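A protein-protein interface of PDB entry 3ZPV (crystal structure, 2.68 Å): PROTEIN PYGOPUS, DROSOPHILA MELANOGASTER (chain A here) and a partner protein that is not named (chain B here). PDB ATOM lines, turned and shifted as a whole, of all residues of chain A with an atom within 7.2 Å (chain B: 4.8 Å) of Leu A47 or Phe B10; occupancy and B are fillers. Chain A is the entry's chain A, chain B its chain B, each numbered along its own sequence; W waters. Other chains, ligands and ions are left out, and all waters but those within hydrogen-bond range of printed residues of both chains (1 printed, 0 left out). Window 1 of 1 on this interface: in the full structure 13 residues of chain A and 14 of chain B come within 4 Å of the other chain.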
ATOM      1  N   VAL A  22     -10.951  17.323 -18.362  1.00  0.00           N
ATOM      2  CA  VAL A  22      -9.920  18.333 -18.493  1.00  0.00           C
ATOM      3  C   VAL A  22      -8.877  18.117 -17.429  1.00  0.00           C
ATOM      4  O   VAL A  22      -9.024  17.272 -16.532  1.00  0.00           O
ATOM      5  CB  VAL A  22     -10.472  19.746 -18.382  1.00  0.00           C
ATOM      6  CG1 VAL A  22     -11.378  20.036 -19.567  1.00  0.00           C
ATOM      7  CG2 VAL A  22     -11.228  19.952 -17.073  1.00  0.00           C
ATOM      8  N   LEU A  39     -18.337  22.996 -17.154  1.00  0.00           N
ATOM      9  CA  LEU A  39     -17.906  23.407 -18.476  1.00  0.00           C
ATOM     10  C   LEU A  39     -18.992  22.990 -19.453  1.00  0.00           C
ATOM     11  O   LEU A  39     -19.449  21.845 -19.426  1.00  0.00           O
ATOM     12  CB  LEU A  39     -16.598  22.687 -18.806  1.00  0.00           C
ATOM     13  CG  LEU A  39     -15.355  23.411 -19.327  1.00  0.00           C
ATOM     14  CD1 LEU A  39     -15.235  24.869 -18.913  1.00  0.00           C
ATOM     15  CD2 LEU A  39     -14.121  22.647 -18.873  1.00  0.00           C
ATOM     16  N   THR A  40     -19.427  23.905 -20.303  1.00  0.00           N
ATOM     17  CA  THR A  40     -20.444  23.569 -21.295  1.00  0.00           C
ATOM     18  C   THR A  40     -19.823  22.705 -22.349  1.00  0.00           C
ATOM     19  O   THR A  40     -18.641  22.728 -22.530  1.00  0.00           O
ATOM     20  CB  THR A  40     -21.038  24.823 -21.982  1.00  0.00           C
ATOM     21  OG1 THR A  40     -20.019  25.540 -22.706  1.00  0.00           O
ATOM     22  CG2 THR A  40     -21.707  25.756 -20.941  1.00  0.00           C
ATOM     23  N   GLU A  41     -20.649  21.990 -23.085  1.00  0.00           N
ATOM     24  CA  GLU A  41     -20.170  21.154 -24.156  1.00  0.00           C
ATOM     25  C   GLU A  41     -19.370  21.950 -25.188  1.00  0.00           C
ATOM     26  O   GLU A  41     -18.366  21.482 -25.702  1.00  0.00           O
ATOM     27  CB  GLU A  41     -21.334  20.442 -24.841  1.00  0.00           C
ATOM     28  CG  GLU A  41     -20.991  19.015 -25.229  1.00  0.00           C
ATOM     29  CD  GLU A  41     -22.201  18.214 -25.681  1.00  0.00           C
ATOM     30  OE1 GLU A  41     -23.255  18.281 -25.008  1.00  0.00           O
ATOM     31  OE2 GLU A  41     -22.078  17.518 -26.719  1.00  0.00           O
ATOM     32  N   ALA A  42     -19.818  23.162 -25.475  1.00  0.00           N
ATOM     33  CA  ALA A  42     -19.160  24.010 -26.443  1.00  0.00           C
ATOM     34  C   ALA A  42     -17.817  24.532 -25.932  1.00  0.00           C
ATOM     35  O   ALA A  42     -16.841  24.609 -26.696  1.00  0.00           O
ATOM     36  CB  ALA A  42     -20.063  25.167 -26.815  1.00  0.00           C
ATOM     37  N   ALA A  43     -17.778  24.970 -24.676  1.00  0.00           N
ATOM     38  CA  ALA A  43     -16.538  25.457 -24.088  1.00  0.00           C
ATOM     39  C   ALA A  43     -15.487  24.340 -24.075  1.00  0.00           C
ATOM     40  O   ALA A  43     -14.325  24.569 -24.363  1.00  0.00           O
ATOM     41  CB  ALA A  43     -16.793  25.961 -22.681  1.00  0.00           C
ATOM     42  N   PHE A  44     -15.916  23.129 -23.761  1.00  0.00           N
ATOM     43  CA  PHE A  44     -15.040  21.966 -23.766  1.00  0.00           C
ATOM     44  C   PHE A  44     -14.451  21.693 -25.152  1.00  0.00           C
ATOM     45  O   PHE A  44     -13.245  21.483 -25.277  1.00  0.00           O
ATOM     46  CB  PHE A  44     -15.853  20.775 -23.271  1.00  0.00           C
ATOM     47  CG  PHE A  44     -15.122  19.476 -23.246  1.00  0.00           C
ATOM     48  CD1 PHE A  44     -14.138  19.227 -22.296  1.00  0.00           C
ATOM     49  CD2 PHE A  44     -15.453  18.477 -24.126  1.00  0.00           C
ATOM     50  CE1 PHE A  44     -13.468  18.004 -22.266  1.00  0.00           C
ATOM     51  CE2 PHE A  44     -14.783  17.253 -24.110  1.00  0.00           C
ATOM     52  CZ  PHE A  44     -13.797  17.008 -23.169  1.00  0.00           C
ATOM     53  N   GLN A  45     -15.285  21.753 -26.188  1.00  0.00           N
ATOM     54  CA  GLN A  45     -14.839  21.524 -27.557  1.00  0.00           C
ATOM     55  C   GLN A  45     -13.872  22.588 -28.026  1.00  0.00           C
ATOM     56  O   GLN A  45     -12.918  22.291 -28.720  1.00  0.00           O
ATOM     57  CB  GLN A  45     -16.011  21.506 -28.523  1.00  0.00           C
ATOM     58  CG  GLN A  45     -16.841  20.239 -28.457  1.00  0.00           C
ATOM     59  CD  GLN A  45     -18.256  20.418 -29.007  1.00  0.00           C
ATOM     60  OE1 GLN A  45     -18.624  21.475 -29.516  1.00  0.00           O
ATOM     61  NE2 GLN A  45     -19.058  19.362 -28.904  1.00  0.00           N
ATOM     62  N   MET A  46     -14.116  23.828 -27.614  1.00  0.00           N
ATOM     63  CA  MET A  46     -13.286  24.948 -28.019  1.00  0.00           C
ATOM     64  C   MET A  46     -11.978  24.971 -27.274  1.00  0.00           C
ATOM     65  O   MET A  46     -10.933  25.183 -27.888  1.00  0.00           O
ATOM     66  CB  MET A  46     -14.040  26.264 -27.881  1.00  0.00           C
ATOM     67  CG  MET A  46     -15.065  26.444 -28.980  1.00  0.00           C
ATOM     68  SD  MET A  46     -16.033  27.954 -28.889  1.00  0.00           S
ATOM     69  CE  MET A  46     -17.476  27.461 -29.838  1.00  0.00           C
ATOM     70  N   LEU A  47     -11.978  24.678 -25.973  1.00  0.00           N
ATOM     71  CA  LEU A  47     -10.697  24.517 -25.279  1.00  0.00           C
ATOM     72  C   LEU A  47      -9.855  23.419 -25.923  1.00  0.00           C
ATOM     73  O   LEU A  47      -8.698  23.613 -26.207  1.00  0.00           O
ATOM     74  CB  LEU A  47     -10.903  24.142 -23.821  1.00  0.00           C
ATOM     75  CG  LEU A  47     -11.392  25.262 -22.932  1.00  0.00           C
ATOM     76  CD1 LEU A  47     -11.856  24.716 -21.604  1.00  0.00           C
ATOM     77  CD2 LEU A  47     -10.317  26.296 -22.725  1.00  0.00           C
ATOM     78  N   ASN A  48     -10.450  22.269 -26.161  1.00  0.00           N
ATOM     79  CA  ASN A  48      -9.689  21.176 -26.717  1.00  0.00           C
ATOM     80  C   ASN A  48      -9.114  21.460 -28.120  1.00  0.00           C
ATOM     81  O   ASN A  48      -8.080  20.923 -28.495  1.00  0.00           O
ATOM     82  CB  ASN A  48     -10.563  19.941 -26.755  1.00  0.00           C
ATOM     83  CG  ASN A  48     -10.870  19.420 -25.372  1.00  0.00           C
ATOM     84  OD1 ASN A  48     -10.190  19.753 -24.421  1.00  0.00           O
ATOM     85  ND2 ASN A  48     -11.888  18.567 -25.268  1.00  0.00           N
ATOM     86  N   LYS A  49      -9.792  22.292 -28.876  1.00  0.00           N
ATOM     87  CA  LYS A  49      -9.523  22.443 -30.299  1.00  0.00           C
ATOM     88  C   LYS A  49      -8.456  23.496 -30.512  1.00  0.00           C
ATOM     89  O   LYS A  49      -7.752  23.468 -31.494  1.00  0.00           O
ATOM     90  CB  LYS A  49     -10.874  22.771 -30.982  1.00  0.00           C
ATOM     91  CG  LYS A  49     -10.913  23.355 -32.363  1.00  0.00           C
ATOM     92  CD  LYS A  49     -12.165  24.246 -32.514  1.00  0.00           C
ATOM     93  CE  LYS A  49     -13.248  23.684 -33.423  1.00  0.00           C
ATOM     94  NZ  LYS A  49     -14.608  23.863 -32.837  1.00  0.00           N
ATOM     95  N   GLU A  50      -8.346  24.413 -29.551  1.00  0.00           N
ATOM     96  CA  GLU A  50      -7.475  25.564 -29.633  1.00  0.00           C
ATOM     97  C   GLU A  50      -6.174  25.272 -28.945  1.00  0.00           C
ATOM     98  O   GLU A  50      -6.093  25.237 -27.714  1.00  0.00           O
ATOM     99  CB  GLU A  50      -8.161  26.768 -28.981  1.00  0.00           C
ATOM    100  CG  GLU A  50      -9.359  27.306 -29.790  1.00  0.00           C
ATOM    101  CD  GLU A  50      -8.920  28.077 -31.050  1.00  0.00           C
ATOM    102  OE1 GLU A  50      -8.302  29.145 -30.887  1.00  0.00           O
ATOM    103  OE2 GLU A  50      -9.170  27.671 -32.213  1.00  0.00           O
ATOM    104  N   VAL A  51      -5.131  25.069 -29.742  1.00  0.00           N
ATOM    105  CA  VAL A  51      -3.845  24.663 -29.237  1.00  0.00           C
ATOM    106  C   VAL A  51      -3.255  25.705 -28.275  1.00  0.00           C
ATOM    107  O   VAL A  51      -2.464  25.357 -27.391  1.00  0.00           O
ATOM    108  CB  VAL A  51      -2.888  24.303 -30.433  1.00  0.00           C
ATOM    109  CG1 VAL A  51      -2.321  25.556 -31.110  1.00  0.00           C
ATOM    110  CG2 VAL A  51      -1.733  23.395 -30.011  1.00  0.00           C
ATOM    111  N   PHE A  52      -3.607  26.970 -28.435  1.00  0.00           N
ATOM    112  CA  PHE A  52      -3.108  28.027 -27.540  1.00  0.00           C
ATOM    113  C   PHE A  52      -3.852  28.135 -26.215  1.00  0.00           C
ATOM    114  O   PHE A  52      -3.465  28.923 -25.346  1.00  0.00           O
ATOM    115  CB  PHE A  52      -3.124  29.385 -28.237  1.00  0.00           C
ATOM    116  CG  PHE A  52      -2.188  29.465 -29.384  1.00  0.00           C
ATOM    117  CD1 PHE A  52      -0.830  29.289 -29.190  1.00  0.00           C
ATOM    118  CD2 PHE A  52      -2.646  29.700 -30.663  1.00  0.00           C
ATOM    119  CE1 PHE A  52       0.060  29.346 -30.259  1.00  0.00           C
ATOM    120  CE2 PHE A  52      -1.766  29.769 -31.733  1.00  0.00           C
ATOM    121  CZ  PHE A  52      -0.404  29.594 -31.535  1.00  0.00           C
ATOM    122  N   ALA A  53      -4.883  27.327 -26.018  1.00  0.00           N
ATOM    123  CA  ALA A  53      -5.719  27.458 -24.826  1.00  0.00           C
ATOM    124  C   ALA A  53      -5.415  26.400 -23.785  1.00  0.00           C
ATOM    125  O   ALA A  53      -5.038  25.305 -24.106  1.00  0.00           O
ATOM    126  CB  ALA A  53      -7.185  27.394 -25.207  1.00  0.00           C
ATOM    127  N   GLU A  54      -5.603  26.746 -22.523  1.00  0.00           N
ATOM    128  CA  GLU A  54      -5.345  25.842 -21.407  1.00  0.00           C
ATOM    129  C   GLU A  54      -6.403  26.159 -20.314  1.00  0.00           C
ATOM    130  O   GLU A  54      -6.784  27.309 -20.123  1.00  0.00           O
ATOM    131  CB  GLU A  54      -3.912  26.054 -20.937  1.00  0.00           C
ATOM    132  CG  GLU A  54      -3.543  25.414 -19.626  1.00  0.00           C
ATOM    133  CD  GLU A  54      -2.124  25.780 -19.144  1.00  0.00           C
ATOM    134  OE1 GLU A  54      -1.132  25.379 -19.800  1.00  0.00           O
ATOM    135  OE2 GLU A  54      -1.999  26.433 -18.066  1.00  0.00           O
ATOM    136  N   TRP A  55      -6.885  25.127 -19.638  1.00  0.00           N
ATOM    137  CA  TRP A  55      -7.866  25.273 -18.592  1.00  0.00           C
ATOM    138  C   TRP A  55      -7.240  25.271 -17.176  1.00  0.00           C
ATOM    139  O   TRP A  55      -6.158  24.721 -16.954  1.00  0.00           O
ATOM    140  CB  TRP A  55      -8.895  24.155 -18.712  1.00  0.00           C
ATOM    141  CG  TRP A  55      -9.938  24.188 -17.655  1.00  0.00           C
ATOM    142  CD1 TRP A  55     -11.026  24.992 -17.608  1.00  0.00           C
ATOM    143  CD2 TRP A  55      -9.984  23.375 -16.473  1.00  0.00           C
ATOM    144  NE1 TRP A  55     -11.751  24.737 -16.475  1.00  0.00           N
ATOM    145  CE2 TRP A  55     -11.131  23.755 -15.753  1.00  0.00           C
ATOM    146  CE3 TRP A  55      -9.157  22.369 -15.945  1.00  0.00           C
ATOM    147  CZ2 TRP A  55     -11.476  23.170 -14.537  1.00  0.00           C
ATOM    148  CZ3 TRP A  55      -9.500  21.800 -14.729  1.00  0.00           C
ATOM    149  CH2 TRP A  55     -10.645  22.203 -14.040  1.00  0.00           C
ATOM    150  N   CYS A  56      -7.963  25.857 -16.227  1.00  0.00           N
ATOM    151  CA  CYS A  56      -7.521  25.988 -14.840  1.00  0.00           C
ATOM    152  C   CYS A  56      -8.719  25.824 -13.888  1.00  0.00           C
ATOM    153  O   CYS A  56      -9.778  26.409 -14.116  1.00  0.00           O
ATOM    154  CB  CYS A  56      -6.869  27.370 -14.651  1.00  0.00           C
ATOM    155  SG  CYS A  56      -6.232  27.674 -13.001  1.00  0.00           S
ATOM    156  N   CYS A  57      -8.543  25.063 -12.807  1.00  0.00           N
ATOM    157  CA  CYS A  57      -9.611  24.864 -11.810  1.00  0.00           C
ATOM    158  C   CYS A  57      -9.798  26.116 -10.961  1.00  0.00           C
ATOM    159  O   CYS A  57      -8.966  27.016 -10.993  1.00  0.00           O
ATOM    160  CB  CYS A  57      -9.327  23.659 -10.893  1.00  0.00           C
ATOM    161  SG  CYS A  57      -8.061  23.889  -9.607  1.00  0.00           S
ATOM    162  N   VAL A  61      -6.899  29.234  -9.567  1.00  0.00           N
ATOM    163  CA  VAL A  61      -6.969  30.603 -10.140  1.00  0.00           C
ATOM    164  C   VAL A  61      -6.285  31.617  -9.201  1.00  0.00           C
ATOM    165  O   VAL A  61      -5.469  32.430  -9.644  1.00  0.00           O
ATOM    166  CB  VAL A  61      -8.427  31.039 -10.448  1.00  0.00           C
ATOM    167  CG1 VAL A  61      -8.473  32.511 -10.842  1.00  0.00           C
ATOM    168  CG2 VAL A  61      -9.031  30.181 -11.560  1.00  0.00           C
ATOM    169  N   PHE B   8      -2.926  30.715 -23.194  1.00  0.00           N
ATOM    170  CA  PHE B   8      -3.952  31.544 -22.626  1.00  0.00           C
ATOM    171  C   PHE B   8      -4.755  30.678 -21.694  1.00  0.00           C
ATOM    172  O   PHE B   8      -5.284  29.609 -22.104  1.00  0.00           O
ATOM    173  CB  PHE B   8      -4.813  32.132 -23.718  1.00  0.00           C
ATOM    174  CG  PHE B   8      -4.046  32.981 -24.669  1.00  0.00           C
ATOM    175  CD1 PHE B   8      -3.356  32.405 -25.725  1.00  0.00           C
ATOM    176  CD2 PHE B   8      -3.998  34.363 -24.517  1.00  0.00           C
ATOM    177  CE1 PHE B   8      -2.646  33.186 -26.636  1.00  0.00           C
ATOM    178  CE2 PHE B   8      -3.285  35.154 -25.422  1.00  0.00           C
ATOM    179  CZ  PHE B   8      -2.619  34.562 -26.488  1.00  0.00           C
ATOM    180  N   VAL B   9      -4.853  31.129 -20.440  1.00  0.00           N
ATOM    181  CA  VAL B   9      -5.464  30.335 -19.382  1.00  0.00           C
ATOM    182  C   VAL B   9      -6.925  30.721 -19.187  1.00  0.00           C
ATOM    183  O   VAL B   9      -7.253  31.878 -19.067  1.00  0.00           O
ATOM    184  CB  VAL B   9      -4.721  30.525 -18.073  1.00  0.00           C
ATOM    185  CG1 VAL B   9      -5.387  29.751 -16.952  1.00  0.00           C
ATOM    186  CG2 VAL B   9      -3.277  30.064 -18.208  1.00  0.00           C
ATOM    187  N   PHE B  10      -7.808  29.729 -19.160  1.00  0.00           N
ATOM    188  CA  PHE B  10      -9.230  29.964 -19.011  1.00  0.00           C
ATOM    189  C   PHE B  10      -9.728  29.240 -17.795  1.00  0.00           C
ATOM    190  O   PHE B  10      -9.542  28.017 -17.662  1.00  0.00           O
ATOM    191  CB  PHE B  10     -10.016  29.385 -20.199  1.00  0.00           C
ATOM    192  CG  PHE B  10      -9.811  30.109 -21.502  1.00  0.00           C
ATOM    193  CD1 PHE B  10      -8.684  29.857 -22.275  1.00  0.00           C
ATOM    194  CD2 PHE B  10     -10.760  30.991 -21.974  1.00  0.00           C
ATOM    195  CE1 PHE B  10      -8.503  30.514 -23.478  1.00  0.00           C
ATOM    196  CE2 PHE B  10     -10.580  31.645 -23.170  1.00  0.00           C
ATOM    197  CZ  PHE B  10      -9.449  31.415 -23.927  1.00  0.00           C
ATOM    198  N   SER B  11     -10.435  29.968 -16.930  1.00  0.00           N
ATOM    199  CA  SER B  11     -11.262  29.311 -15.906  1.00  0.00           C
ATOM    200  C   SER B  11     -12.504  28.755 -16.586  1.00  0.00           C
ATOM    201  O   SER B  11     -12.751  29.028 -17.755  1.00  0.00           O
ATOM    202  CB  SER B  11     -11.642  30.308 -14.850  1.00  0.00           C
ATOM    203  OG  SER B  11     -12.508  31.277 -15.400  1.00  0.00           O
ATOM    204  N   THR B  12     -13.256  27.921 -15.894  1.00  0.00           N
ATOM    205  CA  THR B  12     -14.502  27.403 -16.437  1.00  0.00           C
ATOM    206  C   THR B  12     -15.400  28.547 -16.868  1.00  0.00           C
ATOM    207  O   THR B  12     -15.971  28.535 -17.964  1.00  0.00           O
ATOM    208  CB  THR B  12     -15.249  26.545 -15.416  1.00  0.00           C
ATOM    209  OG1 THR B  12     -14.498  25.360 -15.155  1.00  0.00           O
ATOM    210  CG2 THR B  12     -16.675  26.157 -15.920  1.00  0.00           C
ATOM    211  N   LEU B  14     -14.684  31.687 -17.630  1.00  0.00           N
ATOM    212  CA  LEU B  14     -14.137  32.396 -18.781  1.00  0.00           C
ATOM    213  C   LEU B  14     -14.276  31.563 -20.085  1.00  0.00           C
ATOM    214  O   LEU B  14     -14.617  32.105 -21.129  1.00  0.00           O
ATOM    215  CB  LEU B  14     -12.681  32.761 -18.520  1.00  0.00           C
ATOM    216  CG  LEU B  14     -12.105  33.870 -19.397  1.00  0.00           C
ATOM    217  CD1 LEU B  14     -12.833  35.176 -19.144  1.00  0.00           C
ATOM    218  CD2 LEU B  14     -10.615  34.033 -19.129  1.00  0.00           C
ATOM    219  N   ALA B  15     -14.062  30.256 -20.005  1.00  0.00           N
ATOM    220  CA  ALA B  15     -14.225  29.418 -21.178  1.00  0.00           C
ATOM    221  C   ALA B  15     -15.685  29.386 -21.642  1.00  0.00           C
ATOM    222  O   ALA B  15     -15.957  29.404 -22.840  1.00  0.00           O
ATOM    223  CB  ALA B  15     -13.725  28.002 -20.903  1.00  0.00           C
ATOM    224  N   ILE B  30     -12.037  31.556 -29.070  1.00  0.00           N
ATOM    225  CA  ILE B  30     -11.982  31.942 -27.652  1.00  0.00           C
ATOM    226  C   ILE B  30     -10.696  32.689 -27.307  1.00  0.00           C
ATOM    227  O   ILE B  30     -10.642  33.393 -26.306  1.00  0.00           O
ATOM    228  CB  ILE B  30     -12.180  30.754 -26.687  1.00  0.00           C
ATOM    229  CG1 ILE B  30     -11.167  29.634 -26.967  1.00  0.00           C
ATOM    230  CG2 ILE B  30     -13.590  30.224 -26.802  1.00  0.00           C
ATOM    231  CD1 ILE B  30     -11.147  28.569 -25.893  1.00  0.00           C
ATOM    232  N   ILE B  31      -9.660  32.519 -28.122  1.00  0.00           N
ATOM    233  CA  ILE B  31      -8.391  33.230 -27.912  1.00  0.00           C
ATOM    234  C   ILE B  31      -8.599  34.703 -28.186  1.00  0.00           C
ATOM    235  O   ILE B  31      -8.179  35.550 -27.409  1.00  0.00           O
ATOM    236  CB  ILE B  31      -7.247  32.667 -28.789  1.00  0.00           C
ATOM    237  CG1 ILE B  31      -6.978  31.190 -28.474  1.00  0.00           C
ATOM    238  CG2 ILE B  31      -5.966  33.447 -28.578  1.00  0.00           C
ATOM    239  CD1 ILE B  31      -6.704  30.860 -27.020  1.00  0.00           C
ATOM    240  N   HIS B  34     -10.313  36.156 -25.277  1.00  0.00           N
ATOM    241  CA  HIS B  34      -9.413  36.252 -24.125  1.00  0.00           C
ATOM    242  C   HIS B  34      -8.577  37.535 -24.191  1.00  0.00           C
ATOM    243  O   HIS B  34      -8.415  38.204 -23.173  1.00  0.00           O
ATOM    244  CB  HIS B  34      -8.497  35.025 -24.084  1.00  0.00           C
ATOM    245  CG  HIS B  34      -7.766  34.824 -22.792  1.00  0.00           C
ATOM    246  ND1 HIS B  34      -6.705  35.616 -22.400  1.00  0.00           N
ATOM    247  CD2 HIS B  34      -7.918  33.891 -21.823  1.00  0.00           C
ATOM    248  CE1 HIS B  34      -6.249  35.193 -21.232  1.00  0.00           C
ATOM    249  NE2 HIS B  34      -6.964  34.143 -20.863  1.00  0.00           N
HETATM  250  O   HOH W   1     -12.424  26.837 -13.569  1.00  0.00           O
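Printed residues of chain B within 4 Å of Ala A43: Ala B15. Leu A47 touches just these residues of chain B: Phe B10, Ala B15 and Ile B30. Val A61 touches none of the printed residues of chain B. Of the printed residues of chain A, Phe B8 touches Phe A52, Ala A53 and Glu A54. Phe B10 touches just these residues of chain A: Leu A47, Ala A53, Glu A54, Trp A55 and Cys A56. The nearest printed residue of chain B that does not touch Leu A47 is Ser B11 (5.8 Å).
Hydrophobic or aromatic side chains of chain A within 4 Å of the printed part of chain B: Leu A39, Ala A43, Met A46, Leu A47, Phe A52, Ala A53 and Trp A55.
The backbone NH (N) of Phe B8 sits at hydrogen-bond distance from the backbone carbonyl oxygen (O) of Phe A52 (2.9 Å). The backbone NH of Glu A54 sits at hydrogen-bond distance from the backbone carbonyl oxygen of Phe B8, at 2.9 Å. The backbone NH of Phe B10 is in hydrogen-bond range of the backbone carbonyl oxygen of Glu A54 (2.8 Å). The backbone carbonyl oxygen of Phe B10 sits at hydrogen-bond distance from the backbone NH of Cys A56 (3.0 Å). OG1 of Thr B12 lies within hydrogen-bond range of NE1 of Trp A55, 3.1 Å away.
CG2 of Ile B30 touches SD of Met A46 (3.9 Å). Ala B15 touches Leu A47 (CB to CD1, 3.8 Å). Ile B30 touches Leu A47 (CD1 to N, 3.98 Å). Glu A50 touches Ile B31 (OE1 to CG1, 3.4 Å). Phe B10 touches Ala A53 (CE1 to CB, 3.8 Å). Ala A53 touches Ile B31 (CB to CD1, 3.9 Å). Glu A54 touches Val B9. Phe B10 touches Trp A55. Val B9 touches Cys A56. Ser B11 touches Cys A56 (CA to O, 3.7 Å).
Water W1 lies within hydrogen-bond range of N of Thr B12 (2.7 Å) and O of Cys A56 (2.7 Å).
The backbone carbonyl oxygen (O) of Val B9 lies within hydrogen-bond range of a ring nitrogen (NE2) of His B34 (2.9 Å). N of Leu B14 is in hydrogen-bond range of OG of Ser B11 (3.1 Å). OG1 of Thr A40 is in hydrogen-bond range of N of Ala A43 (3.0 Å).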
